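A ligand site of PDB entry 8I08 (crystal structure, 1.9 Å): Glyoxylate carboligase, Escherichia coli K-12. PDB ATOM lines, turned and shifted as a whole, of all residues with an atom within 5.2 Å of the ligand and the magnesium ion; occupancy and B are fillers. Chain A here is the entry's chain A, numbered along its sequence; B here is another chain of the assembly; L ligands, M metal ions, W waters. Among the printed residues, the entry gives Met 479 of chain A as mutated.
The nearest printed residue that does not touch the magnesium ion is Gly 478 (4.01 Å).
N of Gly 446 sits at hydrogen-bond distance from OG of Ser 397 (3.3 Å). The side-chain amide nitrogen (NE2) of Gln 116 of chain B sits at hydrogen-bond distance from the backbone carbonyl oxygen (O) of Ala 419, 2.6 Å away. SD of Met 479 lies close to N of Gly 395. The side-chain hydroxyl of Ser 445 lies within hydrogen-bond range of the side-chain carboxylate of Asp 449 (2.5 Å). O of Gly 420 sits at hydrogen-bond distance from NE2 of Gln 116 of chain B (3.3 Å). N of Ala 475 sits close to OD2 of Asp 447 (3.1 Å).
The magnesium ion is bound by the side-chain amide oxygen (OD1) of Asn 474. The magnesium ion is bound by O3 of the ligand (2.1 Å). The side-chain carboxylate (OD1) of Asp 447 is bound to the magnesium ion (2.1 Å). An oxygen (O5) of the ligand is bound to the magnesium ion. The magnesium ion is bound by O of Tyr 476, 2.2 Å away. Water W3 is bound to the magnesium ion (2.2 Å).
Ile 394 touches the ligand. Gly 395 touches the ligand. CA of Gly 446 touches O2 of the ligand (3.4 Å). Phe 452 touches the ligand. CB of Leu 477 touches C11 of the ligand, 3.7 Å away. Ile 480 touches the ligand (CD1 to C9, 3.6 Å). Val 26 of chain B touches the ligand. Pro 27 of chain B touches the ligand (O to C10, 3.3 Å). Val 52 of chain B touches the ligand. Thr 76 of chain B touches the ligand. Pro 79 of chain B touches the ligand (CG to N2, 3.8 Å). OD2 of Asp 83 of chain B touches C2 of the ligand, at 3.3 Å. Gln 116 of chain B touches the ligand. Hydrophobic or aromatic side chains within 4 Å of the ligand: Ile 394, Leu 396, Leu 422, Phe 448, Phe 452, Leu 477, Met 479, Ile 480, Val 26 of chain B, Val 52 of chain B and Pro 79 of chain B. Of the 33 residues printed, 24 come within 4 Å of the ligand. Along chain A the residues within 4 Å of the ligand span positions 394 to 480. The nearest printed residue that does not touch the ligand is Ala 80 of chain B (4.03 Å).
Water W3 lies within hydrogen-bond range of an oxygen (O6) of the ligand (2.8 Å), the backbone carbonyl oxygen of Val 472 (2.9 Å) and the side-chain amide nitrogen of Asn 474 (3.1 Å). Water W1 lies within hydrogen-bond range of an oxygen (O2) of the ligand (2.5 Å), the backbone carbonyl oxygen of Ile 394 (2.6 Å), the side-chain hydroxyl of Ser 397 (2.8 Å) and the backbone NH of Gly 446 (2.8 Å). Water W4 lies within hydrogen-bond range of the backbone carbonyl oxygen of Val 26 of chain B (2.8 Å), the backbone NH of Thr 76 of chain B (3.0 Å) and a nitrogen (N1) of the ligand (3.0 Å).
N of Asp 447 lies close to O3 of the ligand (3.2 Å). An oxygen (O7) of the ligand sits at hydrogen-bond distance from the backbone NH (N) of Leu 396. N of Ser 397 is in hydrogen-bond range of O6 of the ligand (2.9 Å). An oxygen (O7) of the ligand is in hydrogen-bond range of the backbone NH of Met 479 (2.8 Å). N of Gly 478 is in hydrogen-bond range of O7 of the ligand. O2 of the ligand lies within hydrogen-bond range of N of Phe 448, at 3.5 Å. The backbone NH (N) of Asp 449 lies within hydrogen-bond range of an oxygen (O2) of the ligand (2.9 Å). The backbone carbonyl oxygen of Gly 420 is in hydrogen-bond range of a nitrogen (N3) of the ligand (2.9 Å). The backbone NH of Leu 422 is in hydrogen-bond range of a nitrogen (N2) of the ligand, 3.5 Å away.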
ATOM      1  N   ILE A 394       5.943  -9.967  29.417  1.00  0.00           N
ATOM      2  CA  ILE A 394       7.304  -9.518  29.708  1.00  0.00           C
ATOM      3  C   ILE A 394       8.096  -9.516  28.401  1.00  0.00           C
ATOM      4  O   ILE A 394       7.737 -10.197  27.446  1.00  0.00           O
ATOM      5  CB  ILE A 394       7.957 -10.444  30.777  1.00  0.00           C
ATOM      6  CG1 ILE A 394       9.194  -9.779  31.412  1.00  0.00           C
ATOM      7  CG2 ILE A 394       8.274 -11.809  30.170  1.00  0.00           C
ATOM      8  CD1 ILE A 394       9.712 -10.509  32.643  1.00  0.00           C
ATOM      9  N   GLY A 395       9.209  -8.806  28.405  1.00  0.00           N
ATOM     10  CA  GLY A 395      10.050  -8.596  27.234  1.00  0.00           C
ATOM     11  C   GLY A 395      10.166  -7.112  26.934  1.00  0.00           C
ATOM     12  O   GLY A 395       9.443  -6.285  27.492  1.00  0.00           O
ATOM     13  N   LEU A 396      11.094  -6.781  26.034  1.00  0.00           N
ATOM     14  CA  LEU A 396      11.137  -5.377  25.641  1.00  0.00           C
ATOM     15  C   LEU A 396       9.803  -4.970  25.013  1.00  0.00           C
ATOM     16  O   LEU A 396       9.375  -3.817  25.146  1.00  0.00           O
ATOM     17  CB  LEU A 396      12.298  -5.097  24.691  1.00  0.00           C
ATOM     18  CG  LEU A 396      13.697  -5.387  25.238  1.00  0.00           C
ATOM     19  CD1 LEU A 396      14.801  -4.990  24.220  1.00  0.00           C
ATOM     20  CD2 LEU A 396      13.932  -4.701  26.587  1.00  0.00           C
ATOM     21  N   SER A 397       9.150  -5.924  24.361  1.00  0.00           N
ATOM     22  CA  SER A 397       7.782  -5.760  23.893  1.00  0.00           C
ATOM     23  C   SER A 397       6.899  -5.144  24.973  1.00  0.00           C
ATOM     24  O   SER A 397       6.218  -4.127  24.728  1.00  0.00           O
ATOM     25  CB  SER A 397       7.241  -7.128  23.529  1.00  0.00           C
ATOM     26  OG  SER A 397       7.427  -8.007  24.651  1.00  0.00           O
ATOM     27  N   ALA A 419       5.657 -12.067  38.435  1.00  0.00           N
ATOM     28  CA  ALA A 419       6.289 -13.323  38.034  1.00  0.00           C
ATOM     29  C   ALA A 419       6.642 -13.383  36.553  1.00  0.00           C
ATOM     30  O   ALA A 419       7.595 -14.087  36.194  1.00  0.00           O
ATOM     31  CB  ALA A 419       5.418 -14.526  38.397  1.00  0.00           C
ATOM     32  N   GLY A 420       5.906 -12.685  35.682  1.00  0.00           N
ATOM     33  CA  GLY A 420       6.224 -12.601  34.269  1.00  0.00           C
ATOM     34  C   GLY A 420       6.613 -13.898  33.552  1.00  0.00           C
ATOM     35  O   GLY A 420       7.636 -13.956  32.874  1.00  0.00           O
ATOM     36  N   PRO A 421       5.809 -14.953  33.658  1.00  0.00           N
ATOM     37  CA  PRO A 421       6.153 -16.212  32.939  1.00  0.00           C
ATOM     38  C   PRO A 421       5.868 -16.124  31.450  1.00  0.00           C
ATOM     39  O   PRO A 421       4.706 -16.023  31.030  1.00  0.00           O
ATOM     40  CB  PRO A 421       5.267 -17.261  33.621  1.00  0.00           C
ATOM     41  CG  PRO A 421       4.091 -16.471  34.133  1.00  0.00           C
ATOM     42  CD  PRO A 421       4.588 -15.087  34.456  1.00  0.00           C
ATOM     43  N   LEU A 422       6.905 -16.254  30.644  1.00  0.00           N
ATOM     44  CA  LEU A 422       6.719 -16.282  29.190  1.00  0.00           C
ATOM     45  C   LEU A 422       5.713 -17.370  28.809  1.00  0.00           C
ATOM     46  O   LEU A 422       5.681 -18.422  29.429  1.00  0.00           O
ATOM     47  CB  LEU A 422       8.055 -16.543  28.495  1.00  0.00           C
ATOM     48  CG  LEU A 422       9.077 -15.413  28.547  1.00  0.00           C
ATOM     49  CD1 LEU A 422      10.414 -15.978  28.150  1.00  0.00           C
ATOM     50  CD2 LEU A 422       8.668 -14.286  27.577  1.00  0.00           C
ATOM     51  N   SER A 445       2.810  -9.227  22.523  1.00  0.00           N
ATOM     52  CA  SER A 445       3.870 -10.197  22.791  1.00  0.00           C
ATOM     53  C   SER A 445       5.059  -9.890  21.899  1.00  0.00           C
ATOM     54  O   SER A 445       4.898  -9.440  20.750  1.00  0.00           O
ATOM     55  CB  SER A 445       3.487 -11.670  22.468  1.00  0.00           C
ATOM     56  OG  SER A 445       2.597 -12.234  23.425  1.00  0.00           O
ATOM     57  N   GLY A 446       6.267 -10.151  22.442  1.00  0.00           N
ATOM     58  CA  GLY A 446       7.428 -10.432  21.611  1.00  0.00           C
ATOM     59  C   GLY A 446       7.365 -11.845  21.018  1.00  0.00           C
ATOM     60  O   GLY A 446       6.527 -12.685  21.389  1.00  0.00           O
ATOM     61  N   ASP A 447       8.261 -12.104  20.057  1.00  0.00           N
ATOM     62  CA  ASP A 447       8.198 -13.385  19.352  1.00  0.00           C
ATOM     63  C   ASP A 447       8.462 -14.576  20.277  1.00  0.00           C
ATOM     64  O   ASP A 447       7.822 -15.609  20.138  1.00  0.00           O
ATOM     65  CB  ASP A 447       9.145 -13.396  18.143  1.00  0.00           C
ATOM     66  CG  ASP A 447      10.516 -12.814  18.437  1.00  0.00           C
ATOM     67  OD1 ASP A 447      10.639 -11.763  19.102  1.00  0.00           O
ATOM     68  OD2 ASP A 447      11.506 -13.406  17.958  1.00  0.00           O
ATOM     69  N   PHE A 448       9.357 -14.436  21.260  1.00  0.00           N
ATOM     70  CA  PHE A 448       9.671 -15.584  22.118  1.00  0.00           C
ATOM     71  C   PHE A 448       8.486 -15.928  23.012  1.00  0.00           C
ATOM     72  O   PHE A 448       8.045 -17.086  23.079  1.00  0.00           O
ATOM     73  CB  PHE A 448      10.913 -15.255  22.952  1.00  0.00           C
ATOM     74  CG  PHE A 448      11.643 -16.456  23.547  1.00  0.00           C
ATOM     75  CD1 PHE A 448      12.015 -17.544  22.782  1.00  0.00           C
ATOM     76  CD2 PHE A 448      12.042 -16.429  24.891  1.00  0.00           C
ATOM     77  CE1 PHE A 448      12.739 -18.600  23.318  1.00  0.00           C
ATOM     78  CE2 PHE A 448      12.775 -17.480  25.455  1.00  0.00           C
ATOM     79  CZ  PHE A 448      13.131 -18.581  24.647  1.00  0.00           C
ATOM     80  N   ASP A 449       7.907 -14.911  23.660  1.00  0.00           N
ATOM     81  CA  ASP A 449       6.719 -15.099  24.482  1.00  0.00           C
ATOM     82  C   ASP A 449       5.621 -15.755  23.676  1.00  0.00           C
ATOM     83  O   ASP A 449       4.910 -16.641  24.173  1.00  0.00           O
ATOM     84  CB  ASP A 449       6.263 -13.731  25.016  1.00  0.00           C
ATOM     85  CG  ASP A 449       4.843 -13.729  25.616  1.00  0.00           C
ATOM     86  OD1 ASP A 449       4.482 -14.678  26.356  1.00  0.00           O
ATOM     87  OD2 ASP A 449       4.081 -12.770  25.375  1.00  0.00           O
ATOM     88  N   PHE A 450       5.460 -15.323  22.424  1.00  0.00           N
ATOM     89  CA  PHE A 450       4.396 -15.821  21.555  1.00  0.00           C
ATOM     90  C   PHE A 450       4.580 -17.299  21.263  1.00  0.00           C
ATOM     91  O   PHE A 450       3.595 -18.031  21.151  1.00  0.00           O
ATOM     92  CB  PHE A 450       4.393 -15.004  20.259  1.00  0.00           C
ATOM     93  CG  PHE A 450       3.169 -15.203  19.397  1.00  0.00           C
ATOM     94  CD1 PHE A 450       1.948 -14.668  19.766  1.00  0.00           C
ATOM     95  CD2 PHE A 450       3.249 -15.895  18.217  1.00  0.00           C
ATOM     96  CE1 PHE A 450       0.832 -14.828  18.957  1.00  0.00           C
ATOM     97  CE2 PHE A 450       2.146 -16.062  17.406  1.00  0.00           C
ATOM     98  CZ  PHE A 450       0.937 -15.534  17.772  1.00  0.00           C
ATOM     99  N   PHE A 452       6.086 -19.708  23.230  1.00  0.00           N
ATOM    100  CA  PHE A 452       6.006 -20.666  24.360  1.00  0.00           C
ATOM    101  C   PHE A 452       4.716 -21.493  24.346  1.00  0.00           C
ATOM    102  O   PHE A 452       4.750 -22.728  24.397  1.00  0.00           O
ATOM    103  CB  PHE A 452       6.084 -19.935  25.710  1.00  0.00           C
ATOM    104  CG  PHE A 452       7.457 -19.914  26.353  1.00  0.00           C
ATOM    105  CD1 PHE A 452       8.573 -19.449  25.659  1.00  0.00           C
ATOM    106  CD2 PHE A 452       7.607 -20.310  27.684  1.00  0.00           C
ATOM    107  CE1 PHE A 452       9.818 -19.411  26.281  1.00  0.00           C
ATOM    108  CE2 PHE A 452       8.834 -20.274  28.307  1.00  0.00           C
ATOM    109  CZ  PHE A 452       9.951 -19.820  27.605  1.00  0.00           C
ATOM    110  N   VAL A 472       5.278  -8.324  18.090  1.00  0.00           N
ATOM    111  CA  VAL A 472       6.376  -7.479  17.645  1.00  0.00           C
ATOM    112  C   VAL A 472       7.619  -8.366  17.600  1.00  0.00           C
ATOM    113  O   VAL A 472       8.085  -8.870  18.624  1.00  0.00           O
ATOM    114  CB  VAL A 472       6.526  -6.211  18.516  1.00  0.00           C
ATOM    115  CG1 VAL A 472       5.214  -5.421  18.499  1.00  0.00           C
ATOM    116  CG2 VAL A 472       6.898  -6.486  19.945  1.00  0.00           C
ATOM    117  N   ASN A 474      11.401  -9.309  16.696  1.00  0.00           N
ATOM    118  CA  ASN A 474      12.787  -8.973  16.421  1.00  0.00           C
ATOM    119  C   ASN A 474      13.678 -10.205  16.230  1.00  0.00           C
ATOM    120  O   ASN A 474      14.903 -10.064  16.169  1.00  0.00           O
ATOM    121  CB  ASN A 474      13.351  -8.084  17.547  1.00  0.00           C
ATOM    122  CG  ASN A 474      13.089  -8.661  18.935  1.00  0.00           C
ATOM    123  OD1 ASN A 474      12.902  -9.878  19.101  1.00  0.00           O
ATOM    124  ND2 ASN A 474      13.091  -7.789  19.955  1.00  0.00           N
ATOM    125  N   ALA A 475      13.110 -11.409  16.137  1.00  0.00           N
ATOM    126  CA  ALA A 475      13.889 -12.640  16.071  1.00  0.00           C
ATOM    127  C   ALA A 475      14.974 -12.660  17.156  1.00  0.00           C
ATOM    128  O   ALA A 475      16.116 -13.064  16.918  1.00  0.00           O
ATOM    129  CB  ALA A 475      14.512 -12.849  14.689  1.00  0.00           C
ATOM    130  N   TYR A 476      14.612 -12.212  18.359  1.00  0.00           N
ATOM    131  CA  TYR A 476      15.569 -12.114  19.464  1.00  0.00           C
ATOM    132  C   TYR A 476      14.851 -12.355  20.778  1.00  0.00           C
ATOM    133  O   TYR A 476      13.679 -11.999  20.928  1.00  0.00           O
ATOM    134  CB  TYR A 476      16.184 -10.729  19.567  1.00  0.00           C
ATOM    135  CG  TYR A 476      17.647 -10.536  19.189  1.00  0.00           C
ATOM    136  CD1 TYR A 476      18.673 -10.882  20.058  1.00  0.00           C
ATOM    137  CD2 TYR A 476      17.983  -9.908  17.998  1.00  0.00           C
ATOM    138  CE1 TYR A 476      19.983 -10.661  19.735  1.00  0.00           C
ATOM    139  CE2 TYR A 476      19.296  -9.677  17.662  1.00  0.00           C
ATOM    140  CZ  TYR A 476      20.285 -10.059  18.531  1.00  0.00           C
ATOM    141  OH  TYR A 476      21.602  -9.819  18.195  1.00  0.00           O
ATOM    142  N   LEU A 477      15.557 -12.893  21.776  1.00  0.00           N
ATOM    143  CA  LEU A 477      15.108 -12.633  23.140  1.00  0.00           C
ATOM    144  C   LEU A 477      15.652 -11.241  23.464  1.00  0.00           C
ATOM    145  O   LEU A 477      16.741 -11.087  24.016  1.00  0.00           O
ATOM    146  CB  LEU A 477      15.612 -13.667  24.151  1.00  0.00           C
ATOM    147  CG  LEU A 477      15.842 -15.147  23.852  1.00  0.00           C
ATOM    148  CD1 LEU A 477      15.978 -16.017  25.135  1.00  0.00           C
ATOM    149  CD2 LEU A 477      14.862 -15.735  22.879  1.00  0.00           C
ATOM    150  N   GLY A 478      14.886 -10.192  23.085  1.00  0.00           N
ATOM    151  CA  GLY A 478      15.451  -8.854  23.088  1.00  0.00           C
ATOM    152  C   GLY A 478      15.813  -8.359  24.486  1.00  0.00           C
ATOM    153  O   GLY A 478      16.893  -7.790  24.692  1.00  0.00           O
ATOM    154  N   MET A 479      14.932  -8.582  25.467  1.00  0.00           N
ATOM    155  CA  MET A 479      15.223  -8.136  26.825  1.00  0.00           C
ATOM    156  C   MET A 479      16.541  -8.712  27.324  1.00  0.00           C
ATOM    157  O   MET A 479      17.256  -8.053  28.079  1.00  0.00           O
ATOM    158  CB  MET A 479      14.085  -8.543  27.754  1.00  0.00           C
ATOM    159  CG  MET A 479      14.148  -8.039  29.197  1.00  0.00           C
ATOM    160  SD  MET A 479      12.519  -8.282  29.925  1.00  0.00           S
ATOM    161  CE  MET A 479      12.880  -8.092  31.679  1.00  0.00           C
ATOM    162  N   ILE A 480      16.881  -9.925  26.879  1.00  0.00           N
ATOM    163  CA  ILE A 480      18.041 -10.620  27.413  1.00  0.00           C
ATOM    164  C   ILE A 480      19.291 -10.194  26.680  1.00  0.00           C
ATOM    165  O   ILE A 480      20.343 -10.057  27.300  1.00  0.00           O
ATOM    166  CB  ILE A 480      17.842 -12.142  27.338  1.00  0.00           C
ATOM    167  CG1 ILE A 480      16.476 -12.504  27.909  1.00  0.00           C
ATOM    168  CG2 ILE A 480      18.988 -12.886  28.084  1.00  0.00           C
ATOM    169  CD1 ILE A 480      16.186 -11.896  29.253  1.00  0.00           C
ATOM    170  N   LEU A 495      16.886 -15.847  17.732  1.00  0.00           N
ATOM    171  CA  LEU A 495      15.934 -16.832  17.221  1.00  0.00           C
ATOM    172  C   LEU A 495      15.957 -16.966  15.706  1.00  0.00           C
ATOM    173  O   LEU A 495      15.197 -17.772  15.162  1.00  0.00           O
ATOM    174  CB  LEU A 495      14.518 -16.490  17.686  1.00  0.00           C
ATOM    175  CG  LEU A 495      14.343 -16.638  19.192  1.00  0.00           C
ATOM    176  CD1 LEU A 495      13.085 -15.935  19.632  1.00  0.00           C
ATOM    177  CD2 LEU A 495      14.323 -18.125  19.599  1.00  0.00           C
ATOM    178  N   VAL B  26      17.159 -21.591  28.526  1.00  0.00           N
ATOM    179  CA  VAL B  26      16.624 -20.283  28.162  1.00  0.00           C
ATOM    180  C   VAL B  26      17.312 -19.281  29.075  1.00  0.00           C
ATOM    181  O   VAL B  26      17.140 -19.370  30.300  1.00  0.00           O
ATOM    182  CB  VAL B  26      15.106 -20.250  28.355  1.00  0.00           C
ATOM    183  CG1 VAL B  26      14.553 -18.852  28.013  1.00  0.00           C
ATOM    184  CG2 VAL B  26      14.444 -21.305  27.510  1.00  0.00           C
ATOM    185  N   PRO B  27      18.105 -18.338  28.573  1.00  0.00           N
ATOM    186  CA  PRO B  27      18.778 -17.384  29.468  1.00  0.00           C
ATOM    187  C   PRO B  27      17.809 -16.322  30.001  1.00  0.00           C
ATOM    188  O   PRO B  27      16.686 -16.170  29.517  1.00  0.00           O
ATOM    189  CB  PRO B  27      19.858 -16.761  28.585  1.00  0.00           C
ATOM    190  CG  PRO B  27      19.239 -16.798  27.208  1.00  0.00           C
ATOM    191  CD  PRO B  27      18.469 -18.096  27.153  1.00  0.00           C
ATOM    192  N   GLY B  28      18.279 -15.604  31.023  1.00  0.00           N
ATOM    193  CA  GLY B  28      17.621 -14.408  31.535  1.00  0.00           C
ATOM    194  C   GLY B  28      18.559 -13.678  32.476  1.00  0.00           C
ATOM    195  O   GLY B  28      19.666 -14.144  32.754  1.00  0.00           O
ATOM    196  N   VAL B  52      10.862 -23.209  28.540  1.00  0.00           N
ATOM    197  CA  VAL B  52      11.724 -23.826  29.548  1.00  0.00           C
ATOM    198  C   VAL B  52      11.337 -25.275  29.733  1.00  0.00           C
ATOM    199  O   VAL B  52      12.191 -26.146  29.907  1.00  0.00           O
ATOM    200  CB  VAL B  52      11.654 -23.043  30.876  1.00  0.00           C
ATOM    201  CG1 VAL B  52      12.304 -23.856  32.018  1.00  0.00           C
ATOM    202  CG2 VAL B  52      12.328 -21.703  30.726  1.00  0.00           C
ATOM    203  N   THR B  76      16.439 -19.138  34.186  1.00  0.00           N
ATOM    204  CA  THR B  76      16.610 -17.974  35.039  1.00  0.00           C
ATOM    205  C   THR B  76      15.803 -18.175  36.336  1.00  0.00           C
ATOM    206  O   THR B  76      15.457 -19.299  36.704  1.00  0.00           O
ATOM    207  CB  THR B  76      16.279 -16.704  34.243  1.00  0.00           C
ATOM    208  OG1 THR B  76      16.773 -15.569  34.951  1.00  0.00           O
ATOM    209  CG2 THR B  76      14.757 -16.531  33.994  1.00  0.00           C
ATOM    210  N   PRO B  79       9.750 -17.945  37.249  1.00  0.00           N
ATOM    211  CA  PRO B  79       8.970 -18.961  36.513  1.00  0.00           C
ATOM    212  C   PRO B  79       9.821 -19.917  35.674  1.00  0.00           C
ATOM    213  O   PRO B  79       9.278 -20.920  35.186  1.00  0.00           O
ATOM    214  CB  PRO B  79       8.052 -18.111  35.632  1.00  0.00           C
ATOM    215  CG  PRO B  79       8.855 -16.885  35.354  1.00  0.00           C
ATOM    216  CD  PRO B  79       9.646 -16.607  36.631  1.00  0.00           C
ATOM    217  N   ALA B  80      11.098 -19.637  35.458  1.00  0.00           N
ATOM    218  CA  ALA B  80      11.929 -20.649  34.815  1.00  0.00           C
ATOM    219  C   ALA B  80      11.972 -21.918  35.654  1.00  0.00           C
ATOM    220  O   ALA B  80      11.770 -23.012  35.147  1.00  0.00           O
ATOM    221  CB  ALA B  80      13.344 -20.112  34.570  1.00  0.00           C
ATOM    222  N   ASP B  83       8.765 -23.877  35.770  1.00  0.00           N
ATOM    223  CA  ASP B  83       8.559 -24.573  34.502  1.00  0.00           C
ATOM    224  C   ASP B  83       9.380 -25.860  34.394  1.00  0.00           C
ATOM    225  O   ASP B  83       9.250 -26.555  33.389  1.00  0.00           O
ATOM    226  CB  ASP B  83       8.931 -23.687  33.305  1.00  0.00           C
ATOM    227  CG  ASP B  83       7.831 -22.722  32.906  1.00  0.00           C
ATOM    228  OD1 ASP B  83       6.679 -22.845  33.392  1.00  0.00           O
ATOM    229  OD2 ASP B  83       8.165 -21.822  32.091  1.00  0.00           O
ATOM    230  N   GLN B 116      10.509 -11.578  40.465  1.00  0.00           N
ATOM    231  CA  GLN B 116      10.706 -12.962  39.996  1.00  0.00           C
ATOM    232  C   GLN B 116      11.599 -13.789  40.928  1.00  0.00           C
ATOM    233  O   GLN B 116      12.354 -14.638  40.456  1.00  0.00           O
ATOM    234  CB  GLN B 116      11.282 -13.003  38.571  1.00  0.00           C
ATOM    235  CG  GLN B 116      10.357 -12.417  37.511  1.00  0.00           C
ATOM    236  CD  GLN B 116      10.783 -12.740  36.055  1.00  0.00           C
ATOM    237  OE1 GLN B 116      11.934 -12.529  35.676  1.00  0.00           O
ATOM    238  NE2 GLN B 116       9.842 -13.256  35.267  1.00  0.00           N
HETATM  239  N1  LIG L   1      12.004 -18.027  31.171  1.00  0.00           N
HETATM  240  C1  LIG L   1      10.720 -17.837  31.531  1.00  0.00           C
HETATM  241  C2  LIG L   1       9.854 -19.043  31.669  1.00  0.00           C
HETATM  242  N2  LIG L   1      10.144 -16.651  31.770  1.00  0.00           N
HETATM  243  C3  LIG L   1      10.902 -15.546  31.670  1.00  0.00           C
HETATM  244  N3  LIG L   1      10.314 -14.366  31.938  1.00  0.00           N
HETATM  245  C4  LIG L   1      12.270 -15.632  31.268  1.00  0.00           C
HETATM  246  C5  LIG L   1      12.739 -16.908  31.040  1.00  0.00           C
HETATM  247  C6  LIG L   1      13.176 -14.426  31.131  1.00  0.00           C
HETATM  248  N4  LIG L   1      12.840 -13.507  30.014  1.00  0.00           N
HETATM  249  C7  LIG L   1      12.295 -12.301  30.193  1.00  0.00           C
HETATM  250  S1  LIG L   1      12.088 -11.462  28.744  1.00  0.00           S
HETATM  251  C8  LIG L   1      12.787 -12.767  27.843  1.00  0.00           C
HETATM  252  C9  LIG L   1      13.138 -13.796  28.676  1.00  0.00           C
HETATM  253  C10 LIG L   1      13.776 -15.092  28.291  1.00  0.00           C
HETATM  254  C11 LIG L   1      12.854 -12.685  26.352  1.00  0.00           C
HETATM  255  C12 LIG L   1      11.521 -12.315  25.748  1.00  0.00           C
HETATM  256  O1  LIG L   1      11.634 -12.204  24.311  1.00  0.00           O
HETATM  257  P1  LIG L   1      10.446 -11.728  23.390  1.00  0.00           P
HETATM  258  O2  LIG L   1       9.143 -12.264  23.944  1.00  0.00           O
HETATM  259  O3  LIG L   1      10.845 -12.003  21.989  1.00  0.00           O
HETATM  260  O4  LIG L   1      10.540 -10.201  23.655  1.00  0.00           O
HETATM  261  P2  LIG L   1      11.507  -9.016  23.247  1.00  0.00           P
HETATM  262  O5  LIG L   1      12.412  -9.554  22.182  1.00  0.00           O
HETATM  263  O6  LIG L   1      10.554  -7.880  22.814  1.00  0.00           O
HETATM  264  O7  LIG L   1      12.291  -8.688  24.517  1.00  0.00           O
HETATM  265 MG    MG M   1      11.852 -10.883  20.563  1.00  0.00          MG
HETATM  266  O   HOH W   1       7.403 -10.759  24.975  1.00  0.00           O
HETATM  267  O   HOH W   2      10.627  -5.437  21.164  1.00  0.00           O
HETATM  268  O   HOH W   3      10.345  -9.256  20.408  1.00  0.00           O
HETATM  269  O   HOH W   4      14.728 -19.256  31.762  1.00  0.00           O
